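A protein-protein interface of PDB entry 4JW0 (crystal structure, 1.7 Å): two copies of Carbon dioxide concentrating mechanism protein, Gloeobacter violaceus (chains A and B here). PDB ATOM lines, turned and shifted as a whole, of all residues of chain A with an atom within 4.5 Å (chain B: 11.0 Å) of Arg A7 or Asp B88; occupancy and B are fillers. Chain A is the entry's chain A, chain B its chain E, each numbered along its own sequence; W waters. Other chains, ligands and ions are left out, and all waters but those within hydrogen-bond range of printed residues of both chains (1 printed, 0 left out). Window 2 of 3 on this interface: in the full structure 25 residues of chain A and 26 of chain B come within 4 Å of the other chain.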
ATOM      1  N   ARG A   5      26.987  -5.583  -9.002  1.00  0.00           N
ATOM      2  CA  ARG A   5      25.863  -4.913  -9.639  1.00  0.00           C
ATOM      3  C   ARG A   5      25.590  -3.632  -8.884  1.00  0.00           C
ATOM      4  O   ARG A   5      25.430  -3.658  -7.668  1.00  0.00           O
ATOM      5  CB  ARG A   5      24.613  -5.797  -9.613  1.00  0.00           C
ATOM      6  CG  ARG A   5      23.363  -5.113 -10.155  1.00  0.00           C
ATOM      7  CD  ARG A   5      22.370  -6.124 -10.712  1.00  0.00           C
ATOM      8  NE  ARG A   5      22.040  -7.148  -9.727  1.00  0.00           N
ATOM      9  CZ  ARG A   5      21.863  -8.439 -10.001  1.00  0.00           C
ATOM     10  NH1 ARG A   5      21.975  -8.902 -11.244  1.00  0.00           N
ATOM     11  NH2 ARG A   5      21.567  -9.279  -9.018  1.00  0.00           N
ATOM     12  N   VAL A   6      25.545  -2.512  -9.600  1.00  0.00           N
ATOM     13  CA  VAL A   6      25.250  -1.227  -8.981  1.00  0.00           C
ATOM     14  C   VAL A   6      23.806  -1.220  -8.498  1.00  0.00           C
ATOM     15  O   VAL A   6      22.884  -1.323  -9.303  1.00  0.00           O
ATOM     16  CB  VAL A   6      25.445  -0.057  -9.970  1.00  0.00           C
ATOM     17  CG1 VAL A   6      25.086   1.262  -9.302  1.00  0.00           C
ATOM     18  CG2 VAL A   6      26.873  -0.016 -10.493  1.00  0.00           C
ATOM     19  N   ARG A   7      23.614  -1.086  -7.191  1.00  0.00           N
ATOM     20  CA  ARG A   7      22.277  -1.152  -6.604  1.00  0.00           C
ATOM     21  C   ARG A   7      21.807   0.162  -6.005  1.00  0.00           C
ATOM     22  O   ARG A   7      20.612   0.345  -5.779  1.00  0.00           O
ATOM     23  CB  ARG A   7      22.221  -2.231  -5.529  1.00  0.00           C
ATOM     24  CG  ARG A   7      22.300  -3.639  -6.075  1.00  0.00           C
ATOM     25  CD  ARG A   7      21.373  -4.551  -5.305  1.00  0.00           C
ATOM     26  NE  ARG A   7      19.976  -4.338  -5.674  1.00  0.00           N
ATOM     27  CZ  ARG A   7      18.936  -4.697  -4.924  1.00  0.00           C
ATOM     28  NH1 ARG A   7      19.125  -5.280  -3.746  1.00  0.00           N
ATOM     29  NH2 ARG A   7      17.702  -4.462  -5.350  1.00  0.00           N
ATOM     30  N   GLY A   8      22.733   1.071  -5.735  1.00  0.00           N
ATOM     31  CA  GLY A   8      22.368   2.333  -5.121  1.00  0.00           C
ATOM     32  C   GLY A   8      23.546   3.224  -4.794  1.00  0.00           C
ATOM     33  O   GLY A   8      24.665   3.009  -5.257  1.00  0.00           O
ATOM     34  N   LEU A  26      26.759   1.741  -3.942  1.00  0.00           N
ATOM     35  CA  LEU A  26      26.456   0.491  -3.268  1.00  0.00           C
ATOM     36  C   LEU A  26      26.455  -0.630  -4.298  1.00  0.00           C
ATOM     37  O   LEU A  26      25.601  -0.667  -5.186  1.00  0.00           O
ATOM     38  CB  LEU A  26      25.091   0.560  -2.582  1.00  0.00           C
ATOM     39  CG  LEU A  26      24.655  -0.724  -1.877  1.00  0.00           C
ATOM     40  CD1 LEU A  26      25.709  -1.162  -0.888  1.00  0.00           C
ATOM     41  CD2 LEU A  26      23.314  -0.548  -1.184  1.00  0.00           C
ATOM     42  N   GLN A  28      26.263  -4.702  -5.112  1.00  0.00           N
ATOM     43  CA  GLN A  28      25.904  -6.049  -4.704  1.00  0.00           C
ATOM     44  C   GLN A  28      26.857  -7.027  -5.367  1.00  0.00           C
ATOM     45  O   GLN A  28      27.006  -7.019  -6.584  1.00  0.00           O
ATOM     46  CB  GLN A  28      24.471  -6.354  -5.157  1.00  0.00           C
ATOM     47  CG  GLN A  28      23.913  -7.677  -4.659  1.00  0.00           C
ATOM     48  CD  GLN A  28      22.470  -7.886  -5.084  1.00  0.00           C
ATOM     49  OE1 GLN A  28      22.136  -7.771  -6.267  1.00  0.00           O
ATOM     50  NE2 GLN A  28      21.603  -8.178  -4.120  1.00  0.00           N
ATOM     51  N   LEU A  51      22.788   2.670 -12.321  1.00  0.00           N
ATOM     52  CA  LEU A  51      22.014   1.617 -11.683  1.00  0.00           C
ATOM     53  C   LEU A  51      21.913   0.377 -12.562  1.00  0.00           C
ATOM     54  O   LEU A  51      21.680   0.479 -13.764  1.00  0.00           O
ATOM     55  CB  LEU A  51      20.615   2.141 -11.361  1.00  0.00           C
ATOM     56  CG  LEU A  51      19.823   1.421 -10.272  1.00  0.00           C
ATOM     57  CD1 LEU A  51      20.526   1.520  -8.924  1.00  0.00           C
ATOM     58  CD2 LEU A  51      18.423   2.014 -10.193  1.00  0.00           C
ATOM     59  N   ILE B   3      29.276  -0.593   5.479  1.00  0.00           N
ATOM     60  CA  ILE B   3      28.404   0.153   6.369  1.00  0.00           C
ATOM     61  C   ILE B   3      28.422  -0.496   7.748  1.00  0.00           C
ATOM     62  O   ILE B   3      28.264  -1.712   7.885  1.00  0.00           O
ATOM     63  CB  ILE B   3      26.954   0.162   5.845  1.00  0.00           C
ATOM     64  CG1 ILE B   3      26.901   0.783   4.447  1.00  0.00           C
ATOM     65  CG2 ILE B   3      26.043   0.915   6.810  1.00  0.00           C
ATOM     66  CD1 ILE B   3      25.622   0.482   3.701  1.00  0.00           C
ATOM     67  N   ASP B  31      24.219  -5.142   6.564  1.00  0.00           N
ATOM     68  CA  ASP B  31      24.244  -5.724   5.219  1.00  0.00           C
ATOM     69  C   ASP B  31      23.580  -4.817   4.185  1.00  0.00           C
ATOM     70  O   ASP B  31      23.136  -3.717   4.495  1.00  0.00           O
ATOM     71  CB  ASP B  31      23.641  -7.141   5.194  1.00  0.00           C
ATOM     72  CG  ASP B  31      22.128  -7.160   5.378  1.00  0.00           C
ATOM     73  OD1 ASP B  31      21.454  -6.137   5.124  1.00  0.00           O
ATOM     74  OD2 ASP B  31      21.607  -8.228   5.770  1.00  0.00           O
ATOM     75  N   GLU B  32      23.531  -5.290   2.944  1.00  0.00           N
ATOM     76  CA  GLU B  32      23.046  -4.481   1.828  1.00  0.00           C
ATOM     77  C   GLU B  32      21.545  -4.224   1.898  1.00  0.00           C
ATOM     78  O   GLU B  32      21.018  -3.400   1.149  1.00  0.00           O
ATOM     79  CB  GLU B  32      23.382  -5.155   0.497  1.00  0.00           C
ATOM     80  CG  GLU B  32      22.708  -6.513   0.289  1.00  0.00           C
ATOM     81  CD  GLU B  32      23.501  -7.663   0.879  1.00  0.00           C
ATOM     82  OE1 GLU B  32      24.558  -7.406   1.493  1.00  0.00           O
ATOM     83  OE2 GLU B  32      23.067  -8.825   0.730  1.00  0.00           O
ATOM     84  N   ALA B  33      20.860  -4.940   2.786  1.00  0.00           N
ATOM     85  CA  ALA B  33      19.427  -4.761   2.979  1.00  0.00           C
ATOM     86  C   ALA B  33      19.155  -3.916   4.218  1.00  0.00           C
ATOM     87  O   ALA B  33      18.008  -3.740   4.622  1.00  0.00           O
ATOM     88  CB  ALA B  33      18.743  -6.109   3.104  1.00  0.00           C
ATOM     89  N   GLY B  34      20.218  -3.396   4.824  1.00  0.00           N
ATOM     90  CA  GLY B  34      20.077  -2.533   5.981  1.00  0.00           C
ATOM     91  C   GLY B  34      19.883  -3.294   7.278  1.00  0.00           C
ATOM     92  O   GLY B  34      19.479  -2.712   8.283  1.00  0.00           O
ATOM     93  N   THR B  84      22.125   9.167   3.927  1.00  0.00           N
ATOM     94  CA  THR B  84      21.161   8.363   3.197  1.00  0.00           C
ATOM     95  C   THR B  84      21.815   7.187   2.487  1.00  0.00           C
ATOM     96  O   THR B  84      22.952   7.271   2.018  1.00  0.00           O
ATOM     97  CB  THR B  84      20.382   9.191   2.135  1.00  0.00           C
ATOM     98  OG1 THR B  84      21.287   9.707   1.154  1.00  0.00           O
ATOM     99  CG2 THR B  84      19.633  10.346   2.785  1.00  0.00           C
ATOM    100  N   VAL B  85      21.076   6.089   2.424  1.00  0.00           N
ATOM    101  CA  VAL B  85      21.395   4.995   1.527  1.00  0.00           C
ATOM    102  C   VAL B  85      20.165   4.757   0.670  1.00  0.00           C
ATOM    103  O   VAL B  85      19.057   4.623   1.187  1.00  0.00           O
ATOM    104  CB  VAL B  85      21.729   3.702   2.277  1.00  0.00           C
ATOM    105  CG1 VAL B  85      22.118   2.617   1.290  1.00  0.00           C
ATOM    106  CG2 VAL B  85      22.838   3.933   3.282  1.00  0.00           C
ATOM    107  N   SER B  86      20.357   4.724  -0.641  1.00  0.00           N
ATOM    108  CA  SER B  86      19.256   4.443  -1.548  1.00  0.00           C
ATOM    109  C   SER B  86      19.530   3.141  -2.270  1.00  0.00           C
ATOM    110  O   SER B  86      20.682   2.818  -2.559  1.00  0.00           O
ATOM    111  CB  SER B  86      19.081   5.578  -2.553  1.00  0.00           C
ATOM    112  OG  SER B  86      20.151   5.600  -3.478  1.00  0.00           O
ATOM    113  N   VAL B  87      18.471   2.382  -2.527  1.00  0.00           N
ATOM    114  CA  VAL B  87      18.556   1.172  -3.336  1.00  0.00           C
ATOM    115  C   VAL B  87      17.455   1.220  -4.384  1.00  0.00           C
ATOM    116  O   VAL B  87      16.290   1.434  -4.053  1.00  0.00           O
ATOM    117  CB  VAL B  87      18.371  -0.091  -2.489  1.00  0.00           C
ATOM    118  CG1 VAL B  87      18.417  -1.326  -3.373  1.00  0.00           C
ATOM    119  CG2 VAL B  87      19.432  -0.169  -1.406  1.00  0.00           C
ATOM    120  N   ASP B  88      17.826   1.033  -5.646  1.00  0.00           N
ATOM    121  CA  ASP B  88      16.863   1.083  -6.742  1.00  0.00           C
ATOM    122  C   ASP B  88      16.083   2.397  -6.737  1.00  0.00           C
ATOM    123  O   ASP B  88      14.856   2.405  -6.852  1.00  0.00           O
ATOM    124  CB  ASP B  88      15.894  -0.099  -6.653  1.00  0.00           C
ATOM    125  CG  ASP B  88      16.604  -1.441  -6.713  1.00  0.00           C
ATOM    126  OD1 ASP B  88      17.636  -1.541  -7.411  1.00  0.00           O
ATOM    127  OD2 ASP B  88      16.135  -2.396  -6.059  1.00  0.00           O
ATOM    128  N   ASN B  89      16.804   3.505  -6.604  1.00  0.00           N
ATOM    129  CA  ASN B  89      16.198   4.836  -6.562  1.00  0.00           C
ATOM    130  C   ASN B  89      15.157   5.016  -5.458  1.00  0.00           C
ATOM    131  O   ASN B  89      14.320   5.915  -5.533  1.00  0.00           O
ATOM    132  CB  ASN B  89      15.571   5.181  -7.916  1.00  0.00           C
ATOM    133  CG  ASN B  89      16.554   5.828  -8.862  1.00  0.00           C
ATOM    134  OD1 ASN B  89      17.349   6.678  -8.459  1.00  0.00           O
ATOM    135  ND2 ASN B  89      16.509   5.432 -10.128  1.00  0.00           N
ATOM    136  N   ARG B  90      15.210   4.172  -4.434  1.00  0.00           N
ATOM    137  CA  ARG B  90      14.322   4.318  -3.285  1.00  0.00           C
ATOM    138  C   ARG B  90      15.128   4.348  -1.992  1.00  0.00           C
ATOM    139  O   ARG B  90      16.191   3.735  -1.903  1.00  0.00           O
ATOM    140  CB  ARG B  90      13.318   3.170  -3.231  1.00  0.00           C
ATOM    141  CG  ARG B  90      12.404   3.090  -4.441  1.00  0.00           C
ATOM    142  CD  ARG B  90      11.583   1.809  -4.449  1.00  0.00           C
ATOM    143  NE  ARG B  90      12.427   0.612  -4.491  1.00  0.00           N
ATOM    144  CZ  ARG B  90      12.263  -0.414  -5.326  1.00  0.00           C
ATOM    145  NH1 ARG B  90      11.279  -0.426  -6.218  1.00  0.00           N
ATOM    146  NH2 ARG B  90      13.097  -1.444  -5.265  1.00  0.00           N
ATOM    147  N   PRO B  91      14.624   5.068  -0.981  1.00  0.00           N
ATOM    148  CA  PRO B  91      15.279   5.130   0.328  1.00  0.00           C
ATOM    149  C   PRO B  91      15.366   3.774   1.022  1.00  0.00           C
ATOM    150  O   PRO B  91      14.361   3.077   1.147  1.00  0.00           O
ATOM    151  CB  PRO B  91      14.361   6.060   1.128  1.00  0.00           C
ATOM    152  CG  PRO B  91      13.690   6.891   0.112  1.00  0.00           C
ATOM    153  CD  PRO B  91      13.472   5.983  -1.056  1.00  0.00           C
ATOM    154  N   LEU B  92      16.565   3.405   1.460  1.00  0.00           N
ATOM    155  CA  LEU B  92      16.733   2.266   2.353  1.00  0.00           C
ATOM    156  C   LEU B  92      16.969   2.789   3.761  1.00  0.00           C
ATOM    157  O   LEU B  92      16.452   2.249   4.739  1.00  0.00           O
ATOM    158  CB  LEU B  92      17.918   1.409   1.926  1.00  0.00           C
ATOM    159  CG  LEU B  92      18.264   0.281   2.902  1.00  0.00           C
ATOM    160  CD1 LEU B  92      17.202  -0.815   2.866  1.00  0.00           C
ATOM    161  CD2 LEU B  92      19.644  -0.286   2.615  1.00  0.00           C
ATOM    162  N   TYR B  93      17.764   3.849   3.847  1.00  0.00           N
ATOM    163  CA  TYR B  93      18.106   4.452   5.122  1.00  0.00           C
ATOM    164  C   TYR B  93      18.121   5.964   5.004  1.00  0.00           C
ATOM    165  O   TYR B  93      18.576   6.522   4.002  1.00  0.00           O
ATOM    166  CB  TYR B  93      19.476   3.961   5.604  1.00  0.00           C
ATOM    167  CG  TYR B  93      19.956   4.652   6.859  1.00  0.00           C
ATOM    168  CD1 TYR B  93      19.548   4.220   8.114  1.00  0.00           C
ATOM    169  CD2 TYR B  93      20.816   5.741   6.790  1.00  0.00           C
ATOM    170  CE1 TYR B  93      19.986   4.850   9.265  1.00  0.00           C
ATOM    171  CE2 TYR B  93      21.258   6.381   7.936  1.00  0.00           C
ATOM    172  CZ  TYR B  93      20.837   5.930   9.171  1.00  0.00           C
ATOM    173  OH  TYR B  93      21.269   6.562  10.316  1.00  0.00           O
HETATM  174  O   HOH W   1      19.440  -4.027  -1.017  1.00  0.00           O
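The guanidinium group of Arg A7 is in salt-bridge range of the side-chain carboxylate of Asp B88 (2.7 Å).
N of Arg A7 lies within hydrogen-bond range of O of Leu A26.
The backbone carbonyl oxygen of Gly A8 sits at hydrogen-bond distance from the backbone NH of Leu A26 (2.8 Å).
NH2 of Arg B90 is in salt-bridge range of OD2 of Asp B88 (3.3 Å).
CA of Val B87 touches O of Arg A7, at 3.3 Å.
Ser B86 touches Gly A8 (O to CA, 3.1 Å).
Leu A26 touches Val B87.
CA of Asp B88 touches CD2 of Leu A51, 3.9 Å away.
ND2 of Asn B89 touches CD2 of Leu A51 (3.9 Å).
Arg A7 touches just these residues of chain B: Val B87 and Asp B88.
Of chain A, only Arg A7 and Leu A51 come within 4 Å of Asp B88.
No residue of chain B comes within 4 Å of Val A6.
Of chain B, only Ser B86 (3.1 Å) comes within 4 Å of Gly A8.
Leu A26 touches just one residue of chain B: Val B87.
No residue of chain B comes within 4 Å of Gln A28.
Of the printed residues of chain B, Leu A51 touches Asp B88 (3.9 Å) and Asn B89 (3.9 Å).
Printed residues of chain A within 4 Å of Asn B89: Leu A51.
Printed residues of chain A within 4 Å of Val B87: Arg A7 and Leu A26.
Printed residues of chain A within 4 Å of Ser B86: Gly A8 (3.1 Å).
Asp B31 touches none of the printed residues of chain A.
Tyr B93 touches none of the printed residues of chain A.
The nearest printed residue of chain A that does not touch Asp B88 is Gly A8 (4.8 Å).
Of the 15 printed residues of chain B, 4 touch a printed residue of chain A.
Hydrophobic or aromatic side chains of chain A within 4 Å of the printed part of chain B: Leu A26 and Leu A51.
Among the printed residues, Asp or Glu carboxylates within 4 Å of a Lys or Arg side-chain nitrogen of the other chain: Arg A7 with Asp B88 (2.7 Å).
No position is printed for both chains.
Of the 6 pairs that touch across the chains among the printed residues, none has its exchanged pair printed and touching as well.
Water W1 bridges the backbone carbonyl oxygen of Glu B32 (2.8 Å) and the guanidinium group of Arg A7 (3.0 Å).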
